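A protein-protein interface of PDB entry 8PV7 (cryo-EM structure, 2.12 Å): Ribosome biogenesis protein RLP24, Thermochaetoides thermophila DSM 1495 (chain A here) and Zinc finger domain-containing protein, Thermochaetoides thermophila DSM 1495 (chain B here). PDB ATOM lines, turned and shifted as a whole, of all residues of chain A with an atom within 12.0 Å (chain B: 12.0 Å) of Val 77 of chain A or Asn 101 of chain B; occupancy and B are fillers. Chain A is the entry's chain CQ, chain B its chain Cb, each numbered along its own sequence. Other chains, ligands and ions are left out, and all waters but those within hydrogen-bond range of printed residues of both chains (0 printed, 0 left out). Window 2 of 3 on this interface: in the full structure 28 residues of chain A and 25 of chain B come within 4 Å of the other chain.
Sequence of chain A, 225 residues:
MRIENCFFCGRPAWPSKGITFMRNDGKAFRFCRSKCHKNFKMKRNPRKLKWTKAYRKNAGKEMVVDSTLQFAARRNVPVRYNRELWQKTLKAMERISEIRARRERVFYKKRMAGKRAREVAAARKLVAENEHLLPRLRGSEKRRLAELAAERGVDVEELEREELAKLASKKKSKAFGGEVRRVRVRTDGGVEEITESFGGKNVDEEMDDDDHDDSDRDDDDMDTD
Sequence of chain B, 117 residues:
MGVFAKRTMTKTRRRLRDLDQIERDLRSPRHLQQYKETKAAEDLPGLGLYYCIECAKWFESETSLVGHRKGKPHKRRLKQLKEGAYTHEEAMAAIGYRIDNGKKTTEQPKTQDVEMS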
ATOM      1  N   ARG A   2       1.518   5.198  13.732  1.00  0.00           N
ATOM      2  CA  ARG A   2       1.164   3.840  14.108  1.00  0.00           C
ATOM      3  C   ARG A   2      -0.218   3.511  13.569  1.00  0.00           C
ATOM      4  O   ARG A   2      -1.001   4.398  13.221  1.00  0.00           O
ATOM      5  CB  ARG A   2       1.214   3.649  15.628  1.00  0.00           C
ATOM      6  CG  ARG A   2       0.180   4.449  16.385  1.00  0.00           C
ATOM      7  CD  ARG A   2       0.189   4.127  17.867  1.00  0.00           C
ATOM      8  NE  ARG A   2      -0.391   2.824  18.169  1.00  0.00           N
ATOM      9  CZ  ARG A   2       0.308   1.735  18.452  1.00  0.00           C
ATOM     10  NH1 ARG A   2       1.630   1.748  18.476  1.00  0.00           N
ATOM     11  NH2 ARG A   2      -0.335   0.604  18.720  1.00  0.00           N
ATOM     12  N   GLN A  70       1.117 -13.219  22.052  1.00  0.00           N
ATOM     13  CA  GLN A  70       1.688 -12.561  23.218  1.00  0.00           C
ATOM     14  C   GLN A  70       2.843 -11.635  22.876  1.00  0.00           C
ATOM     15  O   GLN A  70       3.440 -11.053  23.785  1.00  0.00           O
ATOM     16  CB  GLN A  70       2.153 -13.606  24.234  1.00  0.00           C
ATOM     17  CG  GLN A  70       1.073 -14.590  24.636  1.00  0.00           C
ATOM     18  CD  GLN A  70      -0.175 -13.897  25.139  1.00  0.00           C
ATOM     19  OE1 GLN A  70      -0.159 -13.245  26.181  1.00  0.00           O
ATOM     20  NE2 GLN A  70      -1.268 -14.037  24.398  1.00  0.00           N
ATOM     21  N   PHE A  71       3.170 -11.477  21.597  1.00  0.00           N
ATOM     22  CA  PHE A  71       4.326 -10.687  21.203  1.00  0.00           C
ATOM     23  C   PHE A  71       4.003  -9.230  20.913  1.00  0.00           C
ATOM     24  O   PHE A  71       4.911  -8.394  20.956  1.00  0.00           O
ATOM     25  CB  PHE A  71       4.990 -11.306  19.972  1.00  0.00           C
ATOM     26  CG  PHE A  71       5.679 -12.605  20.248  1.00  0.00           C
ATOM     27  CD1 PHE A  71       6.993 -12.625  20.684  1.00  0.00           C
ATOM     28  CD2 PHE A  71       5.023 -13.808  20.060  1.00  0.00           C
ATOM     29  CE1 PHE A  71       7.633 -13.816  20.933  1.00  0.00           C
ATOM     30  CE2 PHE A  71       5.660 -15.001  20.310  1.00  0.00           C
ATOM     31  CZ  PHE A  71       6.966 -15.004  20.748  1.00  0.00           C
ATOM     32  N   ALA A  72       2.751  -8.902  20.617  1.00  0.00           N
ATOM     33  CA  ALA A  72       2.346  -7.538  20.312  1.00  0.00           C
ATOM     34  C   ALA A  72       1.597  -6.956  21.501  1.00  0.00           C
ATOM     35  O   ALA A  72       0.640  -7.561  21.993  1.00  0.00           O
ATOM     36  CB  ALA A  72       1.477  -7.490  19.055  1.00  0.00           C
ATOM     37  N   ALA A  73       2.034  -5.787  21.959  1.00  0.00           N
ATOM     38  CA  ALA A  73       1.438  -5.148  23.121  1.00  0.00           C
ATOM     39  C   ALA A  73       1.667  -3.647  23.040  1.00  0.00           C
ATOM     40  O   ALA A  73       2.508  -3.167  22.279  1.00  0.00           O
ATOM     41  CB  ALA A  73       2.016  -5.701  24.425  1.00  0.00           C
ATOM     42  N   ARG A  74       0.898  -2.908  23.832  1.00  0.00           N
ATOM     43  CA  ARG A  74       1.123  -1.477  23.991  1.00  0.00           C
ATOM     44  C   ARG A  74       2.219  -1.280  25.027  1.00  0.00           C
ATOM     45  O   ARG A  74       1.993  -1.482  26.222  1.00  0.00           O
ATOM     46  CB  ARG A  74      -0.161  -0.767  24.405  1.00  0.00           C
ATOM     47  CG  ARG A  74       0.012   0.726  24.601  1.00  0.00           C
ATOM     48  CD  ARG A  74      -1.276   1.470  24.360  1.00  0.00           C
ATOM     49  NE  ARG A  74      -1.478   2.537  25.329  1.00  0.00           N
ATOM     50  CZ  ARG A  74      -1.232   3.818  25.093  1.00  0.00           C
ATOM     51  NH1 ARG A  74      -0.754   4.227  23.930  1.00  0.00           N
ATOM     52  NH2 ARG A  74      -1.477   4.711  26.045  1.00  0.00           N
ATOM     53  N   ARG A  75       3.405  -0.894  24.572  1.00  0.00           N
ATOM     54  CA  ARG A  75       4.574  -0.787  25.435  1.00  0.00           C
ATOM     55  C   ARG A  75       4.578   0.578  26.107  1.00  0.00           C
ATOM     56  O   ARG A  75       4.879   1.593  25.473  1.00  0.00           O
ATOM     57  CB  ARG A  75       5.854  -1.006  24.635  1.00  0.00           C
ATOM     58  CG  ARG A  75       5.808  -2.208  23.723  1.00  0.00           C
ATOM     59  CD  ARG A  75       5.923  -3.494  24.502  1.00  0.00           C
ATOM     60  NE  ARG A  75       5.780  -4.656  23.635  1.00  0.00           N
ATOM     61  CZ  ARG A  75       5.977  -5.908  24.020  1.00  0.00           C
ATOM     62  NH1 ARG A  75       6.349  -6.200  25.254  1.00  0.00           N
ATOM     63  NH2 ARG A  75       5.795  -6.890  23.144  1.00  0.00           N
ATOM     64  N   ASN A  76       4.258   0.600  27.396  1.00  0.00           N
ATOM     65  CA  ASN A  76       4.238   1.832  28.165  1.00  0.00           C
ATOM     66  C   ASN A  76       5.573   2.146  28.826  1.00  0.00           C
ATOM     67  O   ASN A  76       5.712   3.221  29.415  1.00  0.00           O
ATOM     68  CB  ASN A  76       3.136   1.765  29.224  1.00  0.00           C
ATOM     69  CG  ASN A  76       1.759   1.995  28.638  1.00  0.00           C
ATOM     70  OD1 ASN A  76       1.623   2.546  27.551  1.00  0.00           O
ATOM     71  ND2 ASN A  76       0.732   1.573  29.357  1.00  0.00           N
ATOM     72  N   VAL A  77       6.544   1.244  28.747  1.00  0.00           N
ATOM     73  CA  VAL A  77       7.891   1.482  29.258  1.00  0.00           C
ATOM     74  C   VAL A  77       8.850   1.478  28.075  1.00  0.00           C
ATOM     75  O   VAL A  77       9.131   0.409  27.517  1.00  0.00           O
ATOM     76  CB  VAL A  77       8.285   0.432  30.308  1.00  0.00           C
ATOM     77  CG1 VAL A  77       9.674   0.710  30.846  1.00  0.00           C
ATOM     78  CG2 VAL A  77       7.272   0.413  31.431  1.00  0.00           C
ATOM     79  N   PRO A  78       9.352   2.635  27.647  1.00  0.00           N
ATOM     80  CA  PRO A  78      10.174   2.681  26.433  1.00  0.00           C
ATOM     81  C   PRO A  78      11.540   2.035  26.613  1.00  0.00           C
ATOM     82  O   PRO A  78      12.087   1.963  27.713  1.00  0.00           O
ATOM     83  CB  PRO A  78      10.303   4.182  26.152  1.00  0.00           C
ATOM     84  CG  PRO A  78      10.103   4.822  27.461  1.00  0.00           C
ATOM     85  CD  PRO A  78       9.099   3.980  28.186  1.00  0.00           C
ATOM     86  N   VAL A  79      12.085   1.570  25.496  1.00  0.00           N
ATOM     87  CA  VAL A  79      13.401   0.953  25.427  1.00  0.00           C
ATOM     88  C   VAL A  79      14.300   1.865  24.604  1.00  0.00           C
ATOM     89  O   VAL A  79      13.861   2.433  23.600  1.00  0.00           O
ATOM     90  CB  VAL A  79      13.310  -0.460  24.813  1.00  0.00           C
ATOM     91  CG1 VAL A  79      14.680  -1.101  24.676  1.00  0.00           C
ATOM     92  CG2 VAL A  79      12.399  -1.335  25.651  1.00  0.00           C
ATOM     93  N   ARG A  80      15.539   2.047  25.065  1.00  0.00           N
ATOM     94  CA  ARG A  80      16.520   2.830  24.323  1.00  0.00           C
ATOM     95  C   ARG A  80      16.770   2.213  22.954  1.00  0.00           C
ATOM     96  O   ARG A  80      16.825   0.990  22.812  1.00  0.00           O
ATOM     97  CB  ARG A  80      17.830   2.911  25.107  1.00  0.00           C
ATOM     98  CG  ARG A  80      18.870   3.835  24.498  1.00  0.00           C
ATOM     99  CD  ARG A  80      20.044   4.036  25.433  1.00  0.00           C
ATOM    100  NE  ARG A  80      19.609   4.423  26.767  1.00  0.00           N
ATOM    101  CZ  ARG A  80      19.400   5.672  27.155  1.00  0.00           C
ATOM    102  NH1 ARG A  80      19.596   6.692  26.339  1.00  0.00           N
ATOM    103  NH2 ARG A  80      18.981   5.902  28.395  1.00  0.00           N
ATOM    104  N   TYR A  81      16.914   3.069  21.943  1.00  0.00           N
ATOM    105  CA  TYR A  81      17.024   2.593  20.572  1.00  0.00           C
ATOM    106  C   TYR A  81      18.321   1.822  20.359  1.00  0.00           C
ATOM    107  O   TYR A  81      19.399   2.266  20.762  1.00  0.00           O
ATOM    108  CB  TYR A  81      16.948   3.753  19.582  1.00  0.00           C
ATOM    109  CG  TYR A  81      17.299   3.328  18.176  1.00  0.00           C
ATOM    110  CD1 TYR A  81      16.485   2.443  17.479  1.00  0.00           C
ATOM    111  CD2 TYR A  81      18.451   3.783  17.557  1.00  0.00           C
ATOM    112  CE1 TYR A  81      16.804   2.036  16.209  1.00  0.00           C
ATOM    113  CE2 TYR A  81      18.775   3.383  16.281  1.00  0.00           C
ATOM    114  CZ  TYR A  81      17.948   2.511  15.612  1.00  0.00           C
ATOM    115  OH  TYR A  81      18.267   2.113  14.339  1.00  0.00           O
ATOM    116  N   ASN A  82      18.200   0.667  19.712  1.00  0.00           N
ATOM    117  CA  ASN A  82      19.326  -0.200  19.396  1.00  0.00           C
ATOM    118  C   ASN A  82      19.072  -0.782  18.017  1.00  0.00           C
ATOM    119  O   ASN A  82      18.041  -1.430  17.798  1.00  0.00           O
ATOM    120  CB  ASN A  82      19.478  -1.304  20.448  1.00  0.00           C
ATOM    121  CG  ASN A  82      20.812  -2.011  20.369  1.00  0.00           C
ATOM    122  OD1 ASN A  82      21.204  -2.516  19.320  1.00  0.00           O
ATOM    123  ND2 ASN A  82      21.522  -2.045  21.485  1.00  0.00           N
ATOM    124  N   LEU A  85      18.737  -4.604  17.856  1.00  0.00           N
ATOM    125  CA  LEU A  85      17.479  -5.020  18.461  1.00  0.00           C
ATOM    126  C   LEU A  85      16.312  -4.772  17.518  1.00  0.00           C
ATOM    127  O   LEU A  85      15.428  -5.624  17.382  1.00  0.00           O
ATOM    128  CB  LEU A  85      17.267  -4.294  19.790  1.00  0.00           C
ATOM    129  CG  LEU A  85      15.900  -4.495  20.450  1.00  0.00           C
ATOM    130  CD1 LEU A  85      15.700  -5.951  20.818  1.00  0.00           C
ATOM    131  CD2 LEU A  85      15.735  -3.609  21.669  1.00  0.00           C
ATOM    132  N   TRP A  86      16.315  -3.632  16.824  1.00  0.00           N
ATOM    133  CA  TRP A  86      15.238  -3.341  15.879  1.00  0.00           C
ATOM    134  C   TRP A  86      15.262  -4.288  14.680  1.00  0.00           C
ATOM    135  O   TRP A  86      14.203  -4.741  14.221  1.00  0.00           O
ATOM    136  CB  TRP A  86      15.315  -1.884  15.428  1.00  0.00           C
ATOM    137  CG  TRP A  86      14.252  -1.015  16.036  1.00  0.00           C
ATOM    138  CD1 TRP A  86      13.155  -0.513  15.408  1.00  0.00           C
ATOM    139  CD2 TRP A  86      14.190  -0.544  17.387  1.00  0.00           C
ATOM    140  NE1 TRP A  86      12.410   0.236  16.279  1.00  0.00           N
ATOM    141  CE2 TRP A  86      13.023   0.235  17.501  1.00  0.00           C
ATOM    142  CE3 TRP A  86      15.003  -0.707  18.510  1.00  0.00           C
ATOM    143  CZ2 TRP A  86      12.652   0.850  18.691  1.00  0.00           C
ATOM    144  CZ3 TRP A  86      14.632  -0.097  19.689  1.00  0.00           C
ATOM    145  CH2 TRP A  86      13.467   0.672  19.772  1.00  0.00           C
ATOM    146  N   GLU B  89     -11.490  -2.314  27.016  1.00  0.00           N
ATOM    147  CA  GLU B  89     -10.848  -3.569  27.393  1.00  0.00           C
ATOM    148  C   GLU B  89     -11.375  -4.730  26.558  1.00  0.00           C
ATOM    149  O   GLU B  89     -10.593  -5.561  26.078  1.00  0.00           O
ATOM    150  CB  GLU B  89     -11.044  -3.853  28.887  1.00  0.00           C
ATOM    151  CG  GLU B  89     -10.695  -2.717  29.866  1.00  0.00           C
ATOM    152  CD  GLU B  89     -11.763  -1.634  29.980  1.00  0.00           C
ATOM    153  OE1 GLU B  89     -11.945  -0.862  29.014  1.00  0.00           O
ATOM    154  OE2 GLU B  89     -12.421  -1.555  31.039  1.00  0.00           O
ATOM    155  N   MET B  92      -9.968  -4.363  23.046  1.00  0.00           N
ATOM    156  CA  MET B  92      -8.586  -4.826  22.960  1.00  0.00           C
ATOM    157  C   MET B  92      -8.505  -6.347  22.988  1.00  0.00           C
ATOM    158  O   MET B  92      -7.723  -6.955  22.241  1.00  0.00           O
ATOM    159  CB  MET B  92      -7.775  -4.223  24.101  1.00  0.00           C
ATOM    160  CG  MET B  92      -6.462  -3.615  23.681  1.00  0.00           C
ATOM    161  SD  MET B  92      -5.406  -3.209  25.082  1.00  0.00           S
ATOM    162  CE  MET B  92      -6.619  -2.661  26.279  1.00  0.00           C
ATOM    163  N   TYR B  97      -4.974  -7.794  21.661  1.00  0.00           N
ATOM    164  CA  TYR B  97      -3.996  -6.778  22.003  1.00  0.00           C
ATOM    165  C   TYR B  97      -4.022  -6.564  23.511  1.00  0.00           C
ATOM    166  O   TYR B  97      -5.065  -6.715  24.152  1.00  0.00           O
ATOM    167  CB  TYR B  97      -4.324  -5.486  21.253  1.00  0.00           C
ATOM    168  CG  TYR B  97      -3.264  -4.414  21.240  1.00  0.00           C
ATOM    169  CD1 TYR B  97      -2.000  -4.668  20.729  1.00  0.00           C
ATOM    170  CD2 TYR B  97      -3.549  -3.129  21.675  1.00  0.00           C
ATOM    171  CE1 TYR B  97      -1.039  -3.684  20.690  1.00  0.00           C
ATOM    172  CE2 TYR B  97      -2.596  -2.140  21.641  1.00  0.00           C
ATOM    173  CZ  TYR B  97      -1.344  -2.422  21.146  1.00  0.00           C
ATOM    174  OH  TYR B  97      -0.396  -1.432  21.106  1.00  0.00           O
ATOM    175  N   ARG B  98      -2.872  -6.224  24.083  1.00  0.00           N
ATOM    176  CA  ARG B  98      -2.769  -6.050  25.525  1.00  0.00           C
ATOM    177  C   ARG B  98      -1.918  -4.828  25.830  1.00  0.00           C
ATOM    178  O   ARG B  98      -1.307  -4.228  24.943  1.00  0.00           O
ATOM    179  CB  ARG B  98      -2.183  -7.291  26.205  1.00  0.00           C
ATOM    180  CG  ARG B  98      -0.893  -7.773  25.582  1.00  0.00           C
ATOM    181  CD  ARG B  98      -0.291  -8.924  26.357  1.00  0.00           C
ATOM    182  NE  ARG B  98       1.077  -9.197  25.936  1.00  0.00           N
ATOM    183  CZ  ARG B  98       2.156  -8.811  26.601  1.00  0.00           C
ATOM    184  NH1 ARG B  98       2.067  -8.138  27.735  1.00  0.00           N
ATOM    185  NH2 ARG B  98       3.357  -9.110  26.116  1.00  0.00           N
ATOM    186  N   ILE B  99      -1.878  -4.466  27.108  1.00  0.00           N
ATOM    187  CA  ILE B  99      -1.115  -3.321  27.588  1.00  0.00           C
ATOM    188  C   ILE B  99       0.039  -3.848  28.426  1.00  0.00           C
ATOM    189  O   ILE B  99      -0.172  -4.619  29.369  1.00  0.00           O
ATOM    190  CB  ILE B  99      -1.993  -2.355  28.398  1.00  0.00           C
ATOM    191  CG1 ILE B  99      -3.076  -1.749  27.508  1.00  0.00           C
ATOM    192  CG2 ILE B  99      -1.150  -1.263  29.027  1.00  0.00           C
ATOM    193  CD1 ILE B  99      -4.005  -0.817  28.237  1.00  0.00           C
ATOM    194  N   ASP B 100       1.254  -3.442  28.077  1.00  0.00           N
ATOM    195  CA  ASP B 100       2.455  -3.838  28.799  1.00  0.00           C
ATOM    196  C   ASP B 100       2.883  -2.645  29.647  1.00  0.00           C
ATOM    197  O   ASP B 100       3.309  -1.618  29.109  1.00  0.00           O
ATOM    198  CB  ASP B 100       3.552  -4.255  27.816  1.00  0.00           C
ATOM    199  CG  ASP B 100       4.854  -4.704  28.486  1.00  0.00           C
ATOM    200  OD1 ASP B 100       5.029  -4.621  29.721  1.00  0.00           O
ATOM    201  OD2 ASP B 100       5.742  -5.146  27.733  1.00  0.00           O
ATOM    202  N   ASN B 101       2.779  -2.789  30.967  1.00  0.00           N
ATOM    203  CA  ASN B 101       3.144  -1.734  31.904  1.00  0.00           C
ATOM    204  C   ASN B 101       4.421  -2.051  32.668  1.00  0.00           C
ATOM    205  O   ASN B 101       4.680  -1.443  33.709  1.00  0.00           O
ATOM    206  CB  ASN B 101       1.996  -1.471  32.875  1.00  0.00           C
ATOM    207  CG  ASN B 101       0.865  -0.709  32.238  1.00  0.00           C
ATOM    208  OD1 ASN B 101       1.081   0.104  31.342  1.00  0.00           O
ATOM    209  ND2 ASN B 101      -0.352  -0.966  32.690  1.00  0.00           N
ATOM    210  N   GLY B 102       5.224  -2.981  32.171  1.00  0.00           N
ATOM    211  CA  GLY B 102       6.454  -3.354  32.841  1.00  0.00           C
ATOM    212  C   GLY B 102       6.284  -4.510  33.803  1.00  0.00           C
ATOM    213  O   GLY B 102       7.086  -5.441  33.809  1.00  0.00           O
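The backbone carbonyl oxygen (O) of Phe 71 of chain A lies within hydrogen-bond range of the guanidinium group (NH2) of Arg 75 of chain A (2.8 Å). The backbone NH (N) of Gly 102 of chain B sits at hydrogen-bond distance from the side-chain carboxylate (OD1) of Asp 100 of chain B (3.0 Å). O of Met 92 of chain B sits at hydrogen-bond distance from N of Tyr 97 of chain B (2.9 Å).
Among the printed residues, merely in contact across the chains: Asn 76 of chain A with Ile 99 of chain B, Ala 73 of chain A with Arg 98 of chain B, Ala 73 of chain A with Tyr 97 of chain B, Arg 74 of chain A with Ile 99 of chain B, Ala 72 of chain A with Arg 98 of chain B, Val 77 of chain A with Asn 101 of chain B and Ala 73 of chain A with Asp 100 of chain B.
O of Arg 98 of chain B is in hydrogen-bond range of N of Arg 74 of chain A. NH1 of Arg 75 of chain A lies within salt-bridge range of OD2 of Asp 100 of chain B. The backbone carbonyl oxygen (O) of Asp 100 of chain B is in hydrogen-bond range of the backbone NH (N) of Asn 76 of chain A (3.0 Å). The side-chain amide nitrogen (ND2) of Asn 76 of chain A sits at hydrogen-bond distance from the side-chain amide oxygen (OD1) of Asn 101 of chain B (2.5 Å). The backbone NH (N) of Asp 100 of chain B is in hydrogen-bond range of the backbone carbonyl oxygen (O) of Arg 74 of chain A. The backbone NH (N) of Arg 74 of chain A sits close to the side-chain hydroxyl (OH) of Tyr 97 of chain B (3.4 Å). The side-chain hydroxyl (OH) of Tyr 97 of chain B is in hydrogen-bond range of the guanidinium group (NH2) of Arg 2 of chain A. O of Gln 70 of chain A is in hydrogen-bond range of NH2 of Arg 98 of chain B (3.0 Å).
Hydrophobic or aromatic side chains of chain B within 4 Å of the printed part of chain A: Tyr 97 and Ile 99. Among the printed residues, Asp or Glu carboxylates within 4 Å of a Lys or Arg side-chain nitrogen of the other chain: Arg 75 of chain A with Asp 100 of chain B (2.8 Å).
Of the printed residues of chain B, Gln 70 of chain A touches Arg 98. Of the printed residues of chain B, Arg 75 of chain A touches Asp 100. Of chain B, only Ile 99, Asp 100 and Asn 101 come within 4 Å of Asn 76 of chain A. Of chain B, only Asn 101 comes within 4 Å of Val 77 of chain A. No residue of chain B comes within 4 Å of Val 79 of chain A. Printed residues of chain A within 4 Å of Arg 98 of chain B: Gln 70, Ala 72, Ala 73 and Arg 74. The nearest residue of chain A that does not touch Asn 101 of chain B is Arg 74 of chain A (5.0 Å).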
